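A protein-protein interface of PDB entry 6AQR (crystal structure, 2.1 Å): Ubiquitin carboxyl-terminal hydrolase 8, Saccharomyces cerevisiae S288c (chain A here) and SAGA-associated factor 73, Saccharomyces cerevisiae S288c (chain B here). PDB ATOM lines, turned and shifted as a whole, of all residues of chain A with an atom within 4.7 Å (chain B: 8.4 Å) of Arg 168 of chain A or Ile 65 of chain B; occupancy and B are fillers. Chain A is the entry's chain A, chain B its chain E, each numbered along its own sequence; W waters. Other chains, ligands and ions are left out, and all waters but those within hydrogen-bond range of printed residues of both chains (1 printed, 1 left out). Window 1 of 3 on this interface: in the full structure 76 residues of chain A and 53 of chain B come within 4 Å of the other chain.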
ATOM      1  N   PRO A 164      21.013  17.500  10.451  1.00  0.00           N
ATOM      2  CA  PRO A 164      22.246  17.342   9.610  1.00  0.00           C
ATOM      3  C   PRO A 164      23.256  16.448  10.252  1.00  0.00           C
ATOM      4  O   PRO A 164      23.995  15.759   9.555  1.00  0.00           O
ATOM      5  CB  PRO A 164      22.804  18.779   9.439  1.00  0.00           C
ATOM      6  CG  PRO A 164      21.960  19.648  10.347  1.00  0.00           C
ATOM      7  CD  PRO A 164      20.726  18.905  10.829  1.00  0.00           C
ATOM      8  N   TYR A 165      23.241  16.344  11.583  1.00  0.00           N
ATOM      9  CA  TYR A 165      24.156  15.408  12.211  1.00  0.00           C
ATOM     10  C   TYR A 165      23.687  13.954  12.123  1.00  0.00           C
ATOM     11  O   TYR A 165      24.516  13.029  11.825  1.00  0.00           O
ATOM     12  CB  TYR A 165      24.429  15.795  13.673  1.00  0.00           C
ATOM     13  CG  TYR A 165      25.118  17.078  13.839  1.00  0.00           C
ATOM     14  CD1 TYR A 165      26.546  17.108  13.862  1.00  0.00           C
ATOM     15  CD2 TYR A 165      24.384  18.278  13.995  1.00  0.00           C
ATOM     16  CE1 TYR A 165      27.213  18.280  14.021  1.00  0.00           C
ATOM     17  CE2 TYR A 165      25.029  19.502  14.146  1.00  0.00           C
ATOM     18  CZ  TYR A 165      26.472  19.502  14.225  1.00  0.00           C
ATOM     19  OH  TYR A 165      27.186  20.658  14.358  1.00  0.00           O
ATOM     20  N   PHE A 166      22.379  13.716  12.339  1.00  0.00           N
ATOM     21  CA  PHE A 166      21.927  12.421  12.174  1.00  0.00           C
ATOM     22  C   PHE A 166      21.970  11.946  10.684  1.00  0.00           C
ATOM     23  O   PHE A 166      22.191  10.740  10.426  1.00  0.00           O
ATOM     24  CB  PHE A 166      20.493  12.194  12.684  1.00  0.00           C
ATOM     25  CG  PHE A 166      20.094  10.750  12.633  1.00  0.00           C
ATOM     26  CD1 PHE A 166      20.674   9.817  13.508  1.00  0.00           C
ATOM     27  CD2 PHE A 166      19.208  10.305  11.610  1.00  0.00           C
ATOM     28  CE1 PHE A 166      20.383   8.459  13.394  1.00  0.00           C
ATOM     29  CE2 PHE A 166      18.906   8.955  11.503  1.00  0.00           C
ATOM     30  CZ  PHE A 166      19.485   8.026  12.405  1.00  0.00           C
ATOM     31  N   ILE A 167      21.652  12.843   9.745  1.00  0.00           N
ATOM     32  CA  ILE A 167      21.701  12.439   8.323  1.00  0.00           C
ATOM     33  C   ILE A 167      23.152  12.054   7.937  1.00  0.00           C
ATOM     34  O   ILE A 167      23.386  11.000   7.310  1.00  0.00           O
ATOM     35  CB  ILE A 167      21.120  13.541   7.474  1.00  0.00           C
ATOM     36  CG1 ILE A 167      19.598  13.381   7.519  1.00  0.00           C
ATOM     37  CG2 ILE A 167      21.461  13.388   6.013  1.00  0.00           C
ATOM     38  CD1 ILE A 167      19.136  12.015   7.017  1.00  0.00           C
ATOM     39  N   ARG A 168      24.124  12.872   8.331  1.00  0.00           N
ATOM     40  CA  ARG A 168      25.506  12.537   7.988  1.00  0.00           C
ATOM     41  C   ARG A 168      25.887  11.170   8.576  1.00  0.00           C
ATOM     42  O   ARG A 168      26.483  10.305   7.919  1.00  0.00           O
ATOM     43  CB  ARG A 168      26.456  13.652   8.386  1.00  0.00           C
ATOM     44  CG  ARG A 168      27.923  13.337   8.053  1.00  0.00           C
ATOM     45  CD  ARG A 168      28.852  14.451   8.490  1.00  0.00           C
ATOM     46  NE  ARG A 168      28.916  14.562   9.965  1.00  0.00           N
ATOM     47  CZ  ARG A 168      29.848  15.280  10.589  1.00  0.00           C
ATOM     48  NH1 ARG A 168      30.719  15.995   9.895  1.00  0.00           N
ATOM     49  NH2 ARG A 168      29.887  15.362  11.885  1.00  0.00           N
ATOM     50  N   HIS A 169      25.513  10.955   9.824  1.00  0.00           N
ATOM     51  CA  HIS A 169      25.813   9.695  10.498  1.00  0.00           C
ATOM     52  C   HIS A 169      25.216   8.467   9.767  1.00  0.00           C
ATOM     53  O   HIS A 169      25.915   7.487   9.471  1.00  0.00           O
ATOM     54  CB  HIS A 169      25.296   9.789  11.932  1.00  0.00           C
ATOM     55  CG  HIS A 169      25.320   8.495  12.680  1.00  0.00           C
ATOM     56  ND1 HIS A 169      26.470   7.979  13.279  1.00  0.00           N
ATOM     57  CD2 HIS A 169      24.303   7.640  12.992  1.00  0.00           C
ATOM     58  CE1 HIS A 169      26.149   6.869  13.928  1.00  0.00           C
ATOM     59  NE2 HIS A 169      24.848   6.647  13.774  1.00  0.00           N
ATOM     60  N   SER A 170      23.935   8.545   9.439  1.00  0.00           N
ATOM     61  CA  SER A 170      23.242   7.473   8.788  1.00  0.00           C
ATOM     62  C   SER A 170      23.809   7.194   7.384  1.00  0.00           C
ATOM     63  O   SER A 170      23.982   6.042   7.027  1.00  0.00           O
ATOM     64  CB  SER A 170      21.732   7.775   8.655  1.00  0.00           C
ATOM     65  OG  SER A 170      21.060   6.566   8.214  1.00  0.00           O
ATOM     66  N   MET A 171      24.093   8.252   6.616  1.00  0.00           N
ATOM     67  CA  MET A 171      24.529   8.099   5.221  1.00  0.00           C
ATOM     68  C   MET A 171      26.003   7.688   5.158  1.00  0.00           C
ATOM     69  O   MET A 171      26.477   7.166   4.133  1.00  0.00           O
ATOM     70  CB  MET A 171      24.261   9.374   4.415  1.00  0.00           C
ATOM     71  CG  MET A 171      22.770   9.679   4.198  1.00  0.00           C
ATOM     72  SD  MET A 171      22.669  10.807   2.783  1.00  0.00           S
ATOM     73  CE  MET A 171      20.902  11.076   2.642  1.00  0.00           C
ATOM     74  N   SER A 172      26.715   7.910   6.270  1.00  0.00           N
ATOM     75  CA  SER A 172      28.084   7.431   6.385  1.00  0.00           C
ATOM     76  C   SER A 172      28.177   5.929   6.740  1.00  0.00           C
ATOM     77  O   SER A 172      29.270   5.419   6.844  1.00  0.00           O
ATOM     78  CB  SER A 172      28.852   8.278   7.427  1.00  0.00           C
ATOM     79  OG  SER A 172      28.944   9.612   6.978  1.00  0.00           O
ATOM     80  N   ILE A 472      24.428  24.569  16.313  1.00  0.00           N
ATOM     81  CA  ILE A 472      25.418  25.571  16.589  1.00  0.00           C
ATOM     82  C   ILE A 472      25.865  26.202  15.277  1.00  0.00           C
ATOM     83  O   ILE A 472      25.998  25.492  14.264  1.00  0.00           O
ATOM     84  CB  ILE A 472      26.628  25.031  17.423  1.00  0.00           C
ATOM     85  CG1 ILE A 472      27.559  26.155  17.872  1.00  0.00           C
ATOM     86  CG2 ILE A 472      27.381  23.870  16.737  1.00  0.00           C
ATOM     87  CD1 ILE A 472      26.888  27.314  18.658  1.00  0.00           C
ATOM     88  N   LEU B  44      42.084  21.094  11.666  1.00  0.00           N
ATOM     89  CA  LEU B  44      40.854  21.601  11.012  1.00  0.00           C
ATOM     90  C   LEU B  44      40.353  22.883  11.702  1.00  0.00           C
ATOM     91  O   LEU B  44      40.297  22.953  12.913  1.00  0.00           O
ATOM     92  CB  LEU B  44      39.783  20.525  11.019  1.00  0.00           C
ATOM     93  CG  LEU B  44      38.466  20.773  10.250  1.00  0.00           C
ATOM     94  CD1 LEU B  44      38.595  20.627   8.740  1.00  0.00           C
ATOM     95  CD2 LEU B  44      37.420  19.831  10.821  1.00  0.00           C
ATOM     96  N   TYR B  46      37.523  26.323  11.702  1.00  0.00           N
ATOM     97  CA  TYR B  46      36.191  26.814  11.264  1.00  0.00           C
ATOM     98  C   TYR B  46      36.241  28.294  11.160  1.00  0.00           C
ATOM     99  O   TYR B  46      36.794  28.956  12.055  1.00  0.00           O
ATOM    100  CB  TYR B  46      35.185  26.447  12.318  1.00  0.00           C
ATOM    101  CG  TYR B  46      35.176  24.965  12.561  1.00  0.00           C
ATOM    102  CD1 TYR B  46      34.628  24.118  11.613  1.00  0.00           C
ATOM    103  CD2 TYR B  46      35.764  24.411  13.690  1.00  0.00           C
ATOM    104  CE1 TYR B  46      34.620  22.750  11.796  1.00  0.00           C
ATOM    105  CE2 TYR B  46      35.779  23.021  13.871  1.00  0.00           C
ATOM    106  CZ  TYR B  46      35.182  22.220  12.925  1.00  0.00           C
ATOM    107  OH  TYR B  46      35.138  20.857  13.054  1.00  0.00           O
ATOM    108  N   MET B  49      33.894  29.662  14.172  1.00  0.00           N
ATOM    109  CA  MET B  49      33.882  28.934  15.410  1.00  0.00           C
ATOM    110  C   MET B  49      35.244  29.007  16.056  1.00  0.00           C
ATOM    111  O   MET B  49      36.140  28.270  15.669  1.00  0.00           O
ATOM    112  CB  MET B  49      33.347  27.497  15.166  1.00  0.00           C
ATOM    113  CG  MET B  49      31.859  27.447  15.431  1.00  0.00           C
ATOM    114  SD  MET B  49      30.824  26.092  14.842  1.00  0.00           S
ATOM    115  CE  MET B  49      31.898  24.719  14.455  1.00  0.00           C
ATOM    116  N   ALA B  62      33.100  16.799  20.600  1.00  0.00           N
ATOM    117  CA  ALA B  62      31.866  17.312  19.971  1.00  0.00           C
ATOM    118  C   ALA B  62      31.963  17.163  18.460  1.00  0.00           C
ATOM    119  O   ALA B  62      32.979  17.481  17.898  1.00  0.00           O
ATOM    120  CB  ALA B  62      31.598  18.791  20.301  1.00  0.00           C
ATOM    121  N   GLN B  63      30.919  16.614  17.840  1.00  0.00           N
ATOM    122  CA  GLN B  63      30.776  16.668  16.408  1.00  0.00           C
ATOM    123  C   GLN B  63      30.412  18.102  16.029  1.00  0.00           C
ATOM    124  O   GLN B  63      29.583  18.696  16.679  1.00  0.00           O
ATOM    125  CB  GLN B  63      29.664  15.707  16.047  1.00  0.00           C
ATOM    126  CG  GLN B  63      30.119  14.811  14.993  1.00  0.00           C
ATOM    127  CD  GLN B  63      29.211  13.657  14.781  1.00  0.00           C
ATOM    128  OE1 GLN B  63      28.360  13.711  13.929  1.00  0.00           O
ATOM    129  NE2 GLN B  63      29.420  12.600  15.516  1.00  0.00           N
ATOM    130  N   LEU B  64      31.059  18.702  15.031  1.00  0.00           N
ATOM    131  CA  LEU B  64      30.687  20.020  14.578  1.00  0.00           C
ATOM    132  C   LEU B  64      30.558  20.048  13.095  1.00  0.00           C
ATOM    133  O   LEU B  64      31.457  19.585  12.381  1.00  0.00           O
ATOM    134  CB  LEU B  64      31.753  21.034  14.946  1.00  0.00           C
ATOM    135  CG  LEU B  64      31.901  21.167  16.464  1.00  0.00           C
ATOM    136  CD1 LEU B  64      33.331  21.576  16.731  1.00  0.00           C
ATOM    137  CD2 LEU B  64      30.809  22.105  17.024  1.00  0.00           C
ATOM    138  N   ILE B  65      29.452  20.586  12.628  1.00  0.00           N
ATOM    139  CA  ILE B  65      29.316  20.943  11.187  1.00  0.00           C
ATOM    140  C   ILE B  65      29.089  22.446  11.173  1.00  0.00           C
ATOM    141  O   ILE B  65      28.064  22.948  11.685  1.00  0.00           O
ATOM    142  CB  ILE B  65      28.137  20.219  10.528  1.00  0.00           C
ATOM    143  CG1 ILE B  65      28.360  18.714  10.559  1.00  0.00           C
ATOM    144  CG2 ILE B  65      27.950  20.642   9.050  1.00  0.00           C
ATOM    145  CD1 ILE B  65      27.104  17.975  10.123  1.00  0.00           C
ATOM    146  N   GLU B  66      30.042  23.170  10.635  1.00  0.00           N
ATOM    147  CA  GLU B  66      29.864  24.608  10.462  1.00  0.00           C
ATOM    148  C   GLU B  66      28.901  24.784   9.308  1.00  0.00           C
ATOM    149  O   GLU B  66      29.031  24.115   8.247  1.00  0.00           O
ATOM    150  CB  GLU B  66      31.173  25.359  10.155  1.00  0.00           C
ATOM    151  CG  GLU B  66      31.107  26.866  10.447  1.00  0.00           C
ATOM    152  CD  GLU B  66      32.383  27.598  10.049  1.00  0.00           C
ATOM    153  OE1 GLU B  66      33.062  27.186   9.083  1.00  0.00           O
ATOM    154  OE2 GLU B  66      32.735  28.575  10.719  1.00  0.00           O
ATOM    155  N   ASP B  67      27.971  25.703   9.542  1.00  0.00           N
ATOM    156  CA  ASP B  67      26.935  26.039   8.601  1.00  0.00           C
ATOM    157  C   ASP B  67      26.243  24.807   7.951  1.00  0.00           C
ATOM    158  O   ASP B  67      26.293  24.622   6.717  1.00  0.00           O
ATOM    159  CB  ASP B  67      27.438  27.095   7.576  1.00  0.00           C
ATOM    160  CG  ASP B  67      26.264  27.823   6.844  1.00  0.00           C
ATOM    161  OD1 ASP B  67      25.039  27.592   7.145  1.00  0.00           O
ATOM    162  OD2 ASP B  67      26.567  28.616   5.931  1.00  0.00           O
ATOM    163  N   PRO B  68      25.587  23.974   8.772  1.00  0.00           N
ATOM    164  CA  PRO B  68      25.061  22.702   8.206  1.00  0.00           C
ATOM    165  C   PRO B  68      23.956  22.878   7.198  1.00  0.00           C
ATOM    166  O   PRO B  68      23.721  21.939   6.463  1.00  0.00           O
ATOM    167  CB  PRO B  68      24.455  21.976   9.433  1.00  0.00           C
ATOM    168  CG  PRO B  68      24.241  23.042  10.483  1.00  0.00           C
ATOM    169  CD  PRO B  68      25.323  24.111  10.230  1.00  0.00           C
ATOM    170  N   LEU B  69      23.285  24.055   7.135  1.00  0.00           N
ATOM    171  CA  LEU B  69      22.282  24.233   6.080  1.00  0.00           C
ATOM    172  C   LEU B  69      22.739  25.068   4.866  1.00  0.00           C
ATOM    173  O   LEU B  69      21.898  25.576   4.146  1.00  0.00           O
ATOM    174  CB  LEU B  69      20.890  24.755   6.614  1.00  0.00           C
ATOM    175  CG  LEU B  69      20.247  23.884   7.710  1.00  0.00           C
ATOM    176  CD1 LEU B  69      18.903  24.495   8.067  1.00  0.00           C
ATOM    177  CD2 LEU B  69      20.130  22.380   7.374  1.00  0.00           C
ATOM    178  N   ASP B  70      24.041  25.242   4.678  1.00  0.00           N
ATOM    179  CA  ASP B  70      24.487  26.065   3.544  1.00  0.00           C
ATOM    180  C   ASP B  70      24.194  25.368   2.206  1.00  0.00           C
ATOM    181  O   ASP B  70      23.868  26.021   1.270  1.00  0.00           O
ATOM    182  CB  ASP B  70      25.939  26.529   3.681  1.00  0.00           C
ATOM    183  CG  ASP B  70      26.897  25.629   3.013  1.00  0.00           C
ATOM    184  OD1 ASP B  70      27.345  24.669   3.701  1.00  0.00           O
ATOM    185  OD2 ASP B  70      27.205  25.903   1.801  1.00  0.00           O
ATOM    186  N   LYS B  71      24.244  24.039   2.172  1.00  0.00           N
ATOM    187  CA  LYS B  71      23.891  23.291   0.962  1.00  0.00           C
ATOM    188  C   LYS B  71      23.126  22.056   1.290  1.00  0.00           C
ATOM    189  O   LYS B  71      23.210  21.601   2.433  1.00  0.00           O
ATOM    190  CB  LYS B  71      25.125  22.962   0.109  1.00  0.00           C
ATOM    191  CG  LYS B  71      26.179  22.073   0.641  1.00  0.00           C
ATOM    192  CD  LYS B  71      27.326  22.158  -0.400  1.00  0.00           C
ATOM    193  CE  LYS B  71      28.563  21.353  -0.036  1.00  0.00           C
ATOM    194  NZ  LYS B  71      29.175  21.861   1.222  1.00  0.00           N
ATOM    195  N   ILE B  73      22.312  18.153   1.706  1.00  0.00           N
ATOM    196  CA  ILE B  73      23.156  16.993   2.023  1.00  0.00           C
ATOM    197  C   ILE B  73      23.814  16.365   0.717  1.00  0.00           C
ATOM    198  O   ILE B  73      23.136  16.204  -0.306  1.00  0.00           O
ATOM    199  CB  ILE B  73      22.300  15.963   2.829  1.00  0.00           C
ATOM    200  CG1 ILE B  73      22.975  14.588   2.989  1.00  0.00           C
ATOM    201  CG2 ILE B  73      20.884  15.878   2.261  1.00  0.00           C
ATOM    202  CD1 ILE B  73      24.286  14.570   3.804  1.00  0.00           C
ATOM    203  N   GLN B  74      25.110  16.058   0.767  1.00  0.00           N
ATOM    204  CA  GLN B  74      25.817  15.637  -0.434  1.00  0.00           C
ATOM    205  C   GLN B  74      25.948  14.133  -0.460  1.00  0.00           C
ATOM    206  O   GLN B  74      26.659  13.546   0.359  1.00  0.00           O
ATOM    207  CB  GLN B  74      27.184  16.350  -0.600  1.00  0.00           C
ATOM    208  CG  GLN B  74      27.147  17.883  -0.895  1.00  0.00           C
ATOM    209  CD  GLN B  74      26.224  18.330  -2.066  1.00  0.00           C
ATOM    210  OE1 GLN B  74      26.534  18.022  -3.223  1.00  0.00           O
ATOM    211  NE2 GLN B  74      25.111  19.094  -1.779  1.00  0.00           N
ATOM    212  N   PRO B  84      21.339   5.616   0.076  1.00  0.00           N
ATOM    213  CA  PRO B  84      21.958   6.928  -0.001  1.00  0.00           C
ATOM    214  C   PRO B  84      23.299   6.938   0.715  1.00  0.00           C
ATOM    215  O   PRO B  84      23.345   6.631   1.912  1.00  0.00           O
ATOM    216  CB  PRO B  84      20.946   7.864   0.687  1.00  0.00           C
ATOM    217  CG  PRO B  84      20.191   7.027   1.621  1.00  0.00           C
ATOM    218  CD  PRO B  84      20.185   5.618   1.017  1.00  0.00           C
ATOM    219  N   LEU B  85      24.370   7.314   0.000  1.00  0.00           N
ATOM    220  CA  LEU B  85      25.759   7.289   0.573  1.00  0.00           C
ATOM    221  C   LEU B  85      26.451   8.593   0.648  1.00  0.00           C
ATOM    222  O   LEU B  85      26.556   9.281  -0.342  1.00  0.00           O
ATOM    223  CB  LEU B  85      26.659   6.319  -0.186  1.00  0.00           C
ATOM    224  CG  LEU B  85      26.066   4.925  -0.548  1.00  0.00           C
ATOM    225  CD1 LEU B  85      27.018   4.147  -1.465  1.00  0.00           C
ATOM    226  CD2 LEU B  85      25.670   4.088   0.677  1.00  0.00           C
ATOM    227  N   ALA B  86      26.942   8.972   1.848  1.00  0.00           N
ATOM    228  CA  ALA B  86      27.781  10.148   1.998  1.00  0.00           C
ATOM    229  C   ALA B  86      29.066   9.930   1.181  1.00  0.00           C
ATOM    230  O   ALA B  86      29.541   8.764   1.023  1.00  0.00           O
ATOM    231  CB  ALA B  86      28.150  10.444   3.493  1.00  0.00           C
ATOM    232  N   LEU B  87      29.602  11.023   0.637  1.00  0.00           N
ATOM    233  CA  LEU B  87      30.772  10.930  -0.223  1.00  0.00           C
ATOM    234  C   LEU B  87      31.934  10.149   0.382  1.00  0.00           C
ATOM    235  O   LEU B  87      32.506   9.267  -0.277  1.00  0.00           O
ATOM    236  CB  LEU B  87      31.196  12.321  -0.667  1.00  0.00           C
ATOM    237  CG  LEU B  87      30.271  13.223  -1.521  1.00  0.00           C
ATOM    238  CD1 LEU B  87      31.027  14.499  -1.966  1.00  0.00           C
ATOM    239  CD2 LEU B  87      29.668  12.463  -2.714  1.00  0.00           C
ATOM    240  N   THR B  88      32.267  10.420   1.635  1.00  0.00           N
ATOM    241  CA  THR B  88      33.328   9.684   2.330  1.00  0.00           C
ATOM    242  C   THR B  88      33.041   8.185   2.553  1.00  0.00           C
ATOM    243  O   THR B  88      33.944   7.454   2.929  1.00  0.00           O
ATOM    244  CB  THR B  88      33.592  10.299   3.746  1.00  0.00           C
ATOM    245  OG1 THR B  88      32.362  10.302   4.504  1.00  0.00           O
ATOM    246  CG2 THR B  88      34.092  11.683   3.592  1.00  0.00           C
ATOM    247  N   ALA B  89      31.814   7.711   2.356  1.00  0.00           N
ATOM    248  CA  ALA B  89      31.493   6.301   2.574  1.00  0.00           C
ATOM    249  C   ALA B  89      31.373   5.517   1.265  1.00  0.00           C
ATOM    250  O   ALA B  89      31.135   4.318   1.264  1.00  0.00           O
ATOM    251  CB  ALA B  89      30.193   6.168   3.369  1.00  0.00           C
HETATM  252  O   HOH W   1      25.842  22.835  13.558  1.00  0.00           O
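NH2 of Arg 168 of chain A sits at hydrogen-bond distance from OE1 of Gln 63 of chain B (3.0 Å). N of Ile 65 of chain B lies within hydrogen-bond range of OH of Tyr 165 of chain A (2.9 Å). The backbone carbonyl oxygen (O) of Met 171 of chain A lies within hydrogen-bond range of the backbone NH (N) of Ala 86 of chain B (2.9 Å).
The side-chain hydroxyl (OG) of Ser 172 of chain A sits at hydrogen-bond distance from the backbone carbonyl oxygen (O) of Arg 168 of chain A (2.7 Å).
Among the printed residues, merely in contact across the chains: Pro 164 of chain A with Ile 65 of chain B, Pro 164 of chain A with Pro 68 of chain B, Tyr 165 of chain A with Gln 63 of chain B, Tyr 165 of chain A with Leu 64 of chain B, Ile 167 of chain A with Ile 73 of chain B, Arg 168 of chain A with Ile 65 of chain B, Met 171 of chain A with Ile 73 of chain B, Met 171 of chain A with Pro 84 of chain B, Met 171 of chain A with Leu 85 of chain B, Met 171 of chain A with Ala 89 of chain B, Ser 172 of chain A with Ala 86 of chain B, Ser 172 of chain A with Ala 89 of chain B and Ile 472 of chain A with Leu 64 of chain B.
Printed residues of chain B that touch a printed residue of chain A: Gln 63, Leu 64, Ile 65, Pro 68, Ile 73, Pro 84, Leu 85, Ala 86 and Ala 89. Along chain B the printed residues that touch a printed residue of chain A span positions 63 to 89. Among the printed residues, 16 pairs touch across the chains.
Of the printed residues of chain B, Arg 168 of chain A touches Gln 63 and Ile 65. Of chain A, only Pro 164, Tyr 165 and Arg 168 come within 4 Å of Ile 65 of chain B. Printed residues of chain B within 4 Å of Tyr 165 of chain A: Gln 63 (3.6 Å), Leu 64 (3.6 Å) and Ile 65 (2.9 Å). Printed residues of chain A within 4 Å of Ala 89 of chain B: Met 171 and Ser 172. Printed residues of chain A within 4 Å of Pro 84 of chain B: Met 171 (3.8 Å). Ala 62 of chain B touches none of the printed residues of chain A. Tyr 46 of chain B touches none of the printed residues of chain A. The nearest residue of chain A that does not touch Ile 65 of chain B is Ile 472 of chain A (4.2 Å). The nearest printed residue of chain A that does not touch Ile 73 of chain B is Arg 168 of chain A (4.8 Å).
Water W1 lies within hydrogen-bond range of OH of Tyr 165 of chain A, O of Ile 472 of chain A and O of Ile 65 of chain B.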
